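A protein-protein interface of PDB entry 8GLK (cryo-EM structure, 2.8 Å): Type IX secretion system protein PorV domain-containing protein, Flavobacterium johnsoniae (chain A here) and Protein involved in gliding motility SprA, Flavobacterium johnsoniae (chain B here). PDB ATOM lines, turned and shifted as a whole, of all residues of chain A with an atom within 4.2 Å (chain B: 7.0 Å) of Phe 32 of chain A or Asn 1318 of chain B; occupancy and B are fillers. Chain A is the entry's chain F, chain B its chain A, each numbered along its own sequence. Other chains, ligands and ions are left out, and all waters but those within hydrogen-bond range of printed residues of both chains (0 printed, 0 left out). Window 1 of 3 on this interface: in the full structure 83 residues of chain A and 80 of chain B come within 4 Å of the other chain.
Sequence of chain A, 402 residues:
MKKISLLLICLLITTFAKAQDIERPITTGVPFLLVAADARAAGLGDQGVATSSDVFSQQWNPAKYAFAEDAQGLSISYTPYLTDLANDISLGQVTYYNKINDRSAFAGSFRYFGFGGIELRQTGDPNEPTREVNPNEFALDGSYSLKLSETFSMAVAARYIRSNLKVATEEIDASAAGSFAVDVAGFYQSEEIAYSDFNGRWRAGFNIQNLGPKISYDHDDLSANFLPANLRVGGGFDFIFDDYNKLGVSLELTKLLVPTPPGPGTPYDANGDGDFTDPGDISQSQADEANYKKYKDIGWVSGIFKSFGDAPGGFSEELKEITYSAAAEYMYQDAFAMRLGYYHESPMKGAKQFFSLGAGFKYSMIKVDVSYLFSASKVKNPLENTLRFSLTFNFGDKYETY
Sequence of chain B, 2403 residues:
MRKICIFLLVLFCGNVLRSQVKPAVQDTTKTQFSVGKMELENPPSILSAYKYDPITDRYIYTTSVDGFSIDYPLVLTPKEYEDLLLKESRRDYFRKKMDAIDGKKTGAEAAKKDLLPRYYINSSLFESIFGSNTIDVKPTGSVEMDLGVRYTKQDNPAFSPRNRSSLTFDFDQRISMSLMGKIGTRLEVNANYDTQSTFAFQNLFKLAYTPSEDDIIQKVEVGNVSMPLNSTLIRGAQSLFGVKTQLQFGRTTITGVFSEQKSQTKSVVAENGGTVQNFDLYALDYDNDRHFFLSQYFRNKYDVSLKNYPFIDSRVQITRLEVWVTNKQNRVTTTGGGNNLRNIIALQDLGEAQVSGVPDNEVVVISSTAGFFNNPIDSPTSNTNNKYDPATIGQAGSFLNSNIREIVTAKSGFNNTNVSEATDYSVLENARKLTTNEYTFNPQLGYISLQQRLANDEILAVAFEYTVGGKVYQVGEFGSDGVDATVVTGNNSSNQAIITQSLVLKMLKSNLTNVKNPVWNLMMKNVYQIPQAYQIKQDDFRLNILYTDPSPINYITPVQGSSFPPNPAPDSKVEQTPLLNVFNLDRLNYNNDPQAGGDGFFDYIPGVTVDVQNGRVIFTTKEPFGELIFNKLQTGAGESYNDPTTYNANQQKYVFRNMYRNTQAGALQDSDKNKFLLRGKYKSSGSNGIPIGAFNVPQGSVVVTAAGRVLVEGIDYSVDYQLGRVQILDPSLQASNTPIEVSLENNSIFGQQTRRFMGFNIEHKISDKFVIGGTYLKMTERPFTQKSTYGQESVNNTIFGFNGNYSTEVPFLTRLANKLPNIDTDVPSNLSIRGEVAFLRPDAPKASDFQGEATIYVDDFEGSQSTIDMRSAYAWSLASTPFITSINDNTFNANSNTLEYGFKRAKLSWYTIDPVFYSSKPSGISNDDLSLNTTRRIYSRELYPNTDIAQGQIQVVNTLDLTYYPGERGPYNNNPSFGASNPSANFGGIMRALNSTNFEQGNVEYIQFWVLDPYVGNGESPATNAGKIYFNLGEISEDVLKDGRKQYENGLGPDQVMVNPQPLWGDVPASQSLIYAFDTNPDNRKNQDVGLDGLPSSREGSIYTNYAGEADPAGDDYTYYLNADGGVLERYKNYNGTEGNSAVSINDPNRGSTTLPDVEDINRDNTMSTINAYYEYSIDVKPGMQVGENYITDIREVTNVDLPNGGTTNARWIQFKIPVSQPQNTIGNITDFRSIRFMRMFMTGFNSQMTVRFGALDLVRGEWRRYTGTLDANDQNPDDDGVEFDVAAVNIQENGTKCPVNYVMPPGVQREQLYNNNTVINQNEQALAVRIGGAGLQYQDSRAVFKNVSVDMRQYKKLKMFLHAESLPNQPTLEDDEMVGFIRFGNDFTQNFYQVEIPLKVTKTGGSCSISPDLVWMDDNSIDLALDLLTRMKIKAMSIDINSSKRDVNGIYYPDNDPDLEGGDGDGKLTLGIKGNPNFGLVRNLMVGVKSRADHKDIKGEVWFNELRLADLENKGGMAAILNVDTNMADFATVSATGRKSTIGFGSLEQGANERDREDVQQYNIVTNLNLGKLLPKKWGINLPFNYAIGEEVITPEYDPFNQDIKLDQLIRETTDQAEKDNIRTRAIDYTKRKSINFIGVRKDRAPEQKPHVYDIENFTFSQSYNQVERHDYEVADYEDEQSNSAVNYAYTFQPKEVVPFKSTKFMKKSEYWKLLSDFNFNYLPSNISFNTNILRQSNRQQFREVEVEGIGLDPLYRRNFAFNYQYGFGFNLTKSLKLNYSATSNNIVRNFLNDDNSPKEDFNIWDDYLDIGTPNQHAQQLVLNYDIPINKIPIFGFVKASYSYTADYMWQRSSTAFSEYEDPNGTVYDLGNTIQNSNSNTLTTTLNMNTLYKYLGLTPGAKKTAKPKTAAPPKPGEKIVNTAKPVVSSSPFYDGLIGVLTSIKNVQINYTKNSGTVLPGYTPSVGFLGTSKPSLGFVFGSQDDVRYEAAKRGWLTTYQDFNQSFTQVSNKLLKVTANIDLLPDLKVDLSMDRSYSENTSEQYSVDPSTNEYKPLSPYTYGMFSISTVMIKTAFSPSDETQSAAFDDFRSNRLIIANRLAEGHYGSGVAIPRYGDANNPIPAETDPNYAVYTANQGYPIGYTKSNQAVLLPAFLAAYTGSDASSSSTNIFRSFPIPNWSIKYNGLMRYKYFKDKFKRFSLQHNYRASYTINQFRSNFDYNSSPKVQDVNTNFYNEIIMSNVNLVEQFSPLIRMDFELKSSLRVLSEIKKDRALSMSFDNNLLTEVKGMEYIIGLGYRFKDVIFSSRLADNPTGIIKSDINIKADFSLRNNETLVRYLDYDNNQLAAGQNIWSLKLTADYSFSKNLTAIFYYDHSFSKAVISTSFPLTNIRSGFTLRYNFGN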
ATOM      1  N   VAL A  30      -7.807   8.963  28.044  1.00  0.00           N
ATOM      2  CA  VAL A  30      -7.368   8.592  26.693  1.00  0.00           C
ATOM      3  C   VAL A  30      -6.281   7.520  26.729  1.00  0.00           C
ATOM      4  O   VAL A  30      -5.135   7.783  26.338  1.00  0.00           O
ATOM      5  CB  VAL A  30      -6.920   9.824  25.879  1.00  0.00           C
ATOM      6  CG1 VAL A  30      -8.135  10.624  25.435  1.00  0.00           C
ATOM      7  CG2 VAL A  30      -5.955  10.723  26.652  1.00  0.00           C
ATOM      8  N   PRO A  31      -6.591   6.301  27.180  1.00  0.00           N
ATOM      9  CA  PRO A  31      -5.555   5.256  27.245  1.00  0.00           C
ATOM     10  C   PRO A  31      -5.011   4.851  25.886  1.00  0.00           C
ATOM     11  O   PRO A  31      -3.937   4.239  25.825  1.00  0.00           O
ATOM     12  CB  PRO A  31      -6.276   4.088  27.930  1.00  0.00           C
ATOM     13  CG  PRO A  31      -7.717   4.313  27.633  1.00  0.00           C
ATOM     14  CD  PRO A  31      -7.909   5.799  27.605  1.00  0.00           C
ATOM     15  N   PHE A  32      -5.707   5.184  24.796  1.00  0.00           N
ATOM     16  CA  PHE A  32      -5.244   4.811  23.464  1.00  0.00           C
ATOM     17  C   PHE A  32      -3.910   5.456  23.114  1.00  0.00           C
ATOM     18  O   PHE A  32      -3.257   5.021  22.160  1.00  0.00           O
ATOM     19  CB  PHE A  32      -6.301   5.183  22.421  1.00  0.00           C
ATOM     20  CG  PHE A  32      -6.168   6.583  21.892  1.00  0.00           C
ATOM     21  CD1 PHE A  32      -6.573   7.666  22.654  1.00  0.00           C
ATOM     22  CD2 PHE A  32      -5.650   6.816  20.628  1.00  0.00           C
ATOM     23  CE1 PHE A  32      -6.455   8.954  22.171  1.00  0.00           C
ATOM     24  CE2 PHE A  32      -5.529   8.103  20.140  1.00  0.00           C
ATOM     25  CZ  PHE A  32      -5.933   9.173  20.914  1.00  0.00           C
ATOM     26  N   LEU A  33      -3.494   6.482  23.859  1.00  0.00           N
ATOM     27  CA  LEU A  33      -2.171   7.061  23.659  1.00  0.00           C
ATOM     28  C   LEU A  33      -1.057   6.078  23.986  1.00  0.00           C
ATOM     29  O   LEU A  33       0.054   6.222  23.464  1.00  0.00           O
ATOM     30  CB  LEU A  33      -2.011   8.319  24.514  1.00  0.00           C
ATOM     31  CG  LEU A  33      -2.822   9.544  24.096  1.00  0.00           C
ATOM     32  CD1 LEU A  33      -2.547  10.710  25.030  1.00  0.00           C
ATOM     33  CD2 LEU A  33      -2.505   9.916  22.663  1.00  0.00           C
ATOM     34  N   LEU A  34      -1.323   5.086  24.834  1.00  0.00           N
ATOM     35  CA  LEU A  34      -0.305   4.124  25.231  1.00  0.00           C
ATOM     36  C   LEU A  34      -0.206   2.932  24.289  1.00  0.00           C
ATOM     37  O   LEU A  34       0.745   2.152  24.403  1.00  0.00           O
ATOM     38  CB  LEU A  34      -0.580   3.625  26.653  1.00  0.00           C
ATOM     39  CG  LEU A  34      -0.562   4.690  27.751  1.00  0.00           C
ATOM     40  CD1 LEU A  34      -0.938   4.083  29.093  1.00  0.00           C
ATOM     41  CD2 LEU A  34       0.797   5.365  27.824  1.00  0.00           C
ATOM     42  N   VAL A  35      -1.152   2.772  23.371  1.00  0.00           N
ATOM     43  CA  VAL A  35      -1.141   1.645  22.447  1.00  0.00           C
ATOM     44  C   VAL A  35      -0.103   1.898  21.363  1.00  0.00           C
ATOM     45  O   VAL A  35      -0.067   2.978  20.761  1.00  0.00           O
ATOM     46  CB  VAL A  35      -2.536   1.427  21.839  1.00  0.00           C
ATOM     47  CG1 VAL A  35      -2.515   0.268  20.855  1.00  0.00           C
ATOM     48  CG2 VAL A  35      -3.558   1.183  22.936  1.00  0.00           C
ATOM     49  N   TYR A  81      -8.605  -3.784  14.939  1.00  0.00           N
ATOM     50  CA  TYR A  81      -9.274  -4.380  16.084  1.00  0.00           C
ATOM     51  C   TYR A  81     -10.446  -5.212  15.587  1.00  0.00           C
ATOM     52  O   TYR A  81     -11.156  -4.801  14.663  1.00  0.00           O
ATOM     53  CB  TYR A  81      -9.770  -3.310  17.060  1.00  0.00           C
ATOM     54  CG  TYR A  81      -8.676  -2.645  17.861  1.00  0.00           C
ATOM     55  CD1 TYR A  81      -7.981  -1.556  17.353  1.00  0.00           C
ATOM     56  CD2 TYR A  81      -8.343  -3.099  19.129  1.00  0.00           C
ATOM     57  CE1 TYR A  81      -6.984  -0.944  18.082  1.00  0.00           C
ATOM     58  CE2 TYR A  81      -7.348  -2.493  19.866  1.00  0.00           C
ATOM     59  CZ  TYR A  81      -6.672  -1.415  19.339  1.00  0.00           C
ATOM     60  OH  TYR A  81      -5.678  -0.806  20.069  1.00  0.00           O
ATOM     61  N   PHE A 113      -7.782   6.535  16.464  1.00  0.00           N
ATOM     62  CA  PHE A 113      -8.489   5.305  16.789  1.00  0.00           C
ATOM     63  C   PHE A 113      -9.962   5.513  16.471  1.00  0.00           C
ATOM     64  O   PHE A 113     -10.574   6.470  16.958  1.00  0.00           O
ATOM     65  CB  PHE A 113      -8.297   4.933  18.259  1.00  0.00           C
ATOM     66  CG  PHE A 113      -9.134   3.771  18.702  1.00  0.00           C
ATOM     67  CD1 PHE A 113      -8.789   2.478  18.352  1.00  0.00           C
ATOM     68  CD2 PHE A 113     -10.271   3.973  19.466  1.00  0.00           C
ATOM     69  CE1 PHE A 113      -9.560   1.408  18.756  1.00  0.00           C
ATOM     70  CE2 PHE A 113     -11.046   2.907  19.874  1.00  0.00           C
ATOM     71  CZ  PHE A 113     -10.689   1.623  19.519  1.00  0.00           C
ATOM     72  N   GLU A 137     -10.969   8.860  18.568  1.00  0.00           N
ATOM     73  CA  GLU A 137     -10.019   9.499  19.471  1.00  0.00           C
ATOM     74  C   GLU A 137      -8.747   9.755  18.685  1.00  0.00           C
ATOM     75  O   GLU A 137      -8.120   8.805  18.210  1.00  0.00           O
ATOM     76  CB  GLU A 137      -9.726   8.620  20.688  1.00  0.00           C
ATOM     77  CG  GLU A 137     -10.638   8.857  21.871  1.00  0.00           C
ATOM     78  CD  GLU A 137     -10.316   7.950  23.040  1.00  0.00           C
ATOM     79  OE1 GLU A 137      -9.715   6.879  22.811  1.00  0.00           O
ATOM     80  OE2 GLU A 137     -10.664   8.305  24.187  1.00  0.00           O
ATOM     81  N   PHE A 138      -8.357  11.016  18.538  1.00  0.00           N
ATOM     82  CA  PHE A 138      -7.159  11.302  17.767  1.00  0.00           C
ATOM     83  C   PHE A 138      -6.238  12.244  18.525  1.00  0.00           C
ATOM     84  O   PHE A 138      -6.670  13.118  19.280  1.00  0.00           O
ATOM     85  CB  PHE A 138      -7.489  11.873  16.374  1.00  0.00           C
ATOM     86  CG  PHE A 138      -8.048  13.267  16.388  1.00  0.00           C
ATOM     87  CD1 PHE A 138      -7.204  14.366  16.353  1.00  0.00           C
ATOM     88  CD2 PHE A 138      -9.414  13.479  16.404  1.00  0.00           C
ATOM     89  CE1 PHE A 138      -7.710  15.646  16.354  1.00  0.00           C
ATOM     90  CE2 PHE A 138      -9.926  14.758  16.404  1.00  0.00           C
ATOM     91  CZ  PHE A 138      -9.072  15.843  16.378  1.00  0.00           C
ATOM     92  N   ALA A 139      -4.946  12.059  18.280  1.00  0.00           N
ATOM     93  CA  ALA A 139      -3.902  12.906  18.838  1.00  0.00           C
ATOM     94  C   ALA A 139      -3.043  13.412  17.693  1.00  0.00           C
ATOM     95  O   ALA A 139      -2.495  12.615  16.925  1.00  0.00           O
ATOM     96  CB  ALA A 139      -3.050  12.146  19.857  1.00  0.00           C
ATOM     97  N   ILE A 161      -4.870  16.244  22.076  1.00  0.00           N
ATOM     98  CA  ILE A 161      -5.652  15.017  22.153  1.00  0.00           C
ATOM     99  C   ILE A 161      -7.126  15.389  22.169  1.00  0.00           C
ATOM    100  O   ILE A 161      -7.537  16.277  22.926  1.00  0.00           O
ATOM    101  CB  ILE A 161      -5.284  14.191  23.399  1.00  0.00           C
ATOM    102  CG1 ILE A 161      -3.781  13.914  23.434  1.00  0.00           C
ATOM    103  CG2 ILE A 161      -6.065  12.890  23.426  1.00  0.00           C
ATOM    104  CD1 ILE A 161      -3.036  14.726  24.468  1.00  0.00           C
ATOM    105  N   GLN B 951     -12.934   4.685  29.598  1.00  0.00           N
ATOM    106  CA  GLN B 951     -12.541   6.078  29.445  1.00  0.00           C
ATOM    107  C   GLN B 951     -13.092   6.646  28.143  1.00  0.00           C
ATOM    108  O   GLN B 951     -13.051   5.995  27.095  1.00  0.00           O
ATOM    109  CB  GLN B 951     -11.020   6.205  29.480  1.00  0.00           C
ATOM    110  CG  GLN B 951     -10.375   5.546  30.688  1.00  0.00           C
ATOM    111  CD  GLN B 951     -10.776   6.196  31.998  1.00  0.00           C
ATOM    112  OE1 GLN B 951     -11.149   7.368  32.036  1.00  0.00           O
ATOM    113  NE2 GLN B 951     -10.707   5.433  33.082  1.00  0.00           N
ATOM    114  N   TYR B1315     -11.558  -5.961  28.475  1.00  0.00           N
ATOM    115  CA  TYR B1315     -10.983  -4.763  27.874  1.00  0.00           C
ATOM    116  C   TYR B1315     -12.072  -4.062  27.073  1.00  0.00           C
ATOM    117  O   TYR B1315     -12.493  -4.560  26.024  1.00  0.00           O
ATOM    118  CB  TYR B1315      -9.790  -5.113  26.987  1.00  0.00           C
ATOM    119  CG  TYR B1315      -8.451  -4.934  27.662  1.00  0.00           C
ATOM    120  CD1 TYR B1315      -7.882  -3.676  27.796  1.00  0.00           C
ATOM    121  CD2 TYR B1315      -7.753  -6.024  28.164  1.00  0.00           C
ATOM    122  CE1 TYR B1315      -6.658  -3.507  28.412  1.00  0.00           C
ATOM    123  CE2 TYR B1315      -6.529  -5.864  28.782  1.00  0.00           C
ATOM    124  CZ  TYR B1315      -5.987  -4.604  28.903  1.00  0.00           C
ATOM    125  OH  TYR B1315      -4.766  -4.440  29.517  1.00  0.00           O
ATOM    126  N   ASN B1316     -12.527  -2.906  27.561  1.00  0.00           N
ATOM    127  CA  ASN B1316     -13.573  -2.173  26.853  1.00  0.00           C
ATOM    128  C   ASN B1316     -12.989  -1.346  25.713  1.00  0.00           C
ATOM    129  O   ASN B1316     -13.281  -1.597  24.541  1.00  0.00           O
ATOM    130  CB  ASN B1316     -14.341  -1.281  27.830  1.00  0.00           C
ATOM    131  CG  ASN B1316     -15.716  -0.905  27.315  1.00  0.00           C
ATOM    132  OD1 ASN B1316     -15.845  -0.174  26.333  1.00  0.00           O
ATOM    133  ND2 ASN B1316     -16.752  -1.400  27.980  1.00  0.00           N
ATOM    134  N   ASN B1317     -12.153  -0.357  26.043  1.00  0.00           N
ATOM    135  CA  ASN B1317     -11.371   0.414  25.067  1.00  0.00           C
ATOM    136  C   ASN B1317     -10.013   0.684  25.710  1.00  0.00           C
ATOM    137  O   ASN B1317      -9.826   1.707  26.373  1.00  0.00           O
ATOM    138  CB  ASN B1317     -12.069   1.712  24.673  1.00  0.00           C
ATOM    139  CG  ASN B1317     -13.072   1.533  23.550  1.00  0.00           C
ATOM    140  OD1 ASN B1317     -13.171   0.467  22.948  1.00  0.00           O
ATOM    141  ND2 ASN B1317     -13.827   2.587  23.264  1.00  0.00           N
ATOM    142  N   ASN B1318      -9.068  -0.235  25.503  1.00  0.00           N
ATOM    143  CA  ASN B1318      -7.720  -0.141  26.070  1.00  0.00           C
ATOM    144  C   ASN B1318      -7.740   0.041  27.587  1.00  0.00           C
ATOM    145  O   ASN B1318      -6.733   0.437  28.185  1.00  0.00           O
ATOM    146  CB  ASN B1318      -6.919   0.986  25.409  1.00  0.00           C
ATOM    147  CG  ASN B1318      -7.007   0.952  23.898  1.00  0.00           C
ATOM    148  OD1 ASN B1318      -6.778  -0.085  23.277  1.00  0.00           O
ATOM    149  ND2 ASN B1318      -7.344   2.086  23.299  1.00  0.00           N
ATOM    150  N   THR B1319      -8.873  -0.238  28.225  1.00  0.00           N
ATOM    151  CA  THR B1319      -9.035  -0.083  29.662  1.00  0.00           C
ATOM    152  C   THR B1319      -9.510  -1.397  30.260  1.00  0.00           C
ATOM    153  O   THR B1319     -10.289  -2.129  29.641  1.00  0.00           O
ATOM    154  CB  THR B1319     -10.020   1.054  30.000  1.00  0.00           C
ATOM    155  OG1 THR B1319     -10.025   1.287  31.414  1.00  0.00           O
ATOM    156  CG2 THR B1319     -11.430   0.724  29.529  1.00  0.00           C
ATOM    157  N   VAL B1320      -9.017  -1.707  31.456  1.00  0.00           N
ATOM    158  CA  VAL B1320      -9.407  -2.932  32.144  1.00  0.00           C
ATOM    159  C   VAL B1320     -10.673  -2.654  32.944  1.00  0.00           C
ATOM    160  O   VAL B1320     -10.675  -1.822  33.858  1.00  0.00           O
ATOM    161  CB  VAL B1320      -8.279  -3.443  33.050  1.00  0.00           C
ATOM    162  CG1 VAL B1320      -8.745  -4.657  33.837  1.00  0.00           C
ATOM    163  CG2 VAL B1320      -7.049  -3.776  32.225  1.00  0.00           C
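OD1 of Asn 1318 of chain B sits at hydrogen-bond distance from OH of Tyr 81 of chain A (3.5 Å).
Among the printed residues, pairs that only touch across the chains: Phe 32 of chain A with Asn 1318 of chain B, Val 35 of chain A with Asn 1318 of chain B, Pro 31 of chain A with Asn 1317 of chain B, Pro 31 of chain A with Gln 951 of chain B and Pro 31 of chain A with Asn 1318 of chain B.
Of the printed residues of chain B, Pro 31 of chain A touches Gln 951, Asn 1317 and Asn 1318. Of the printed residues of chain B, Phe 32 of chain A touches Asn 1318 (3.4 Å). Printed residues of chain B within 4 Å of Val 35 of chain A: Asn 1318. Of the printed residues of chain A, Gln 951 of chain B touches Pro 31 (3.7 Å). Of the printed residues of chain A, Asn 1317 of chain B touches Pro 31. Val 1320 of chain B touches none of the printed residues of chain A. The nearest residue of chain B that does not touch Phe 32 of chain A is Asn 1317 of chain B (5.6 Å). The nearest printed residue of chain A that does not touch Asn 1318 of chain B is Phe 113 of chain A (5.1 Å).
Among the printed residues, 6 pairs touch across the chains.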
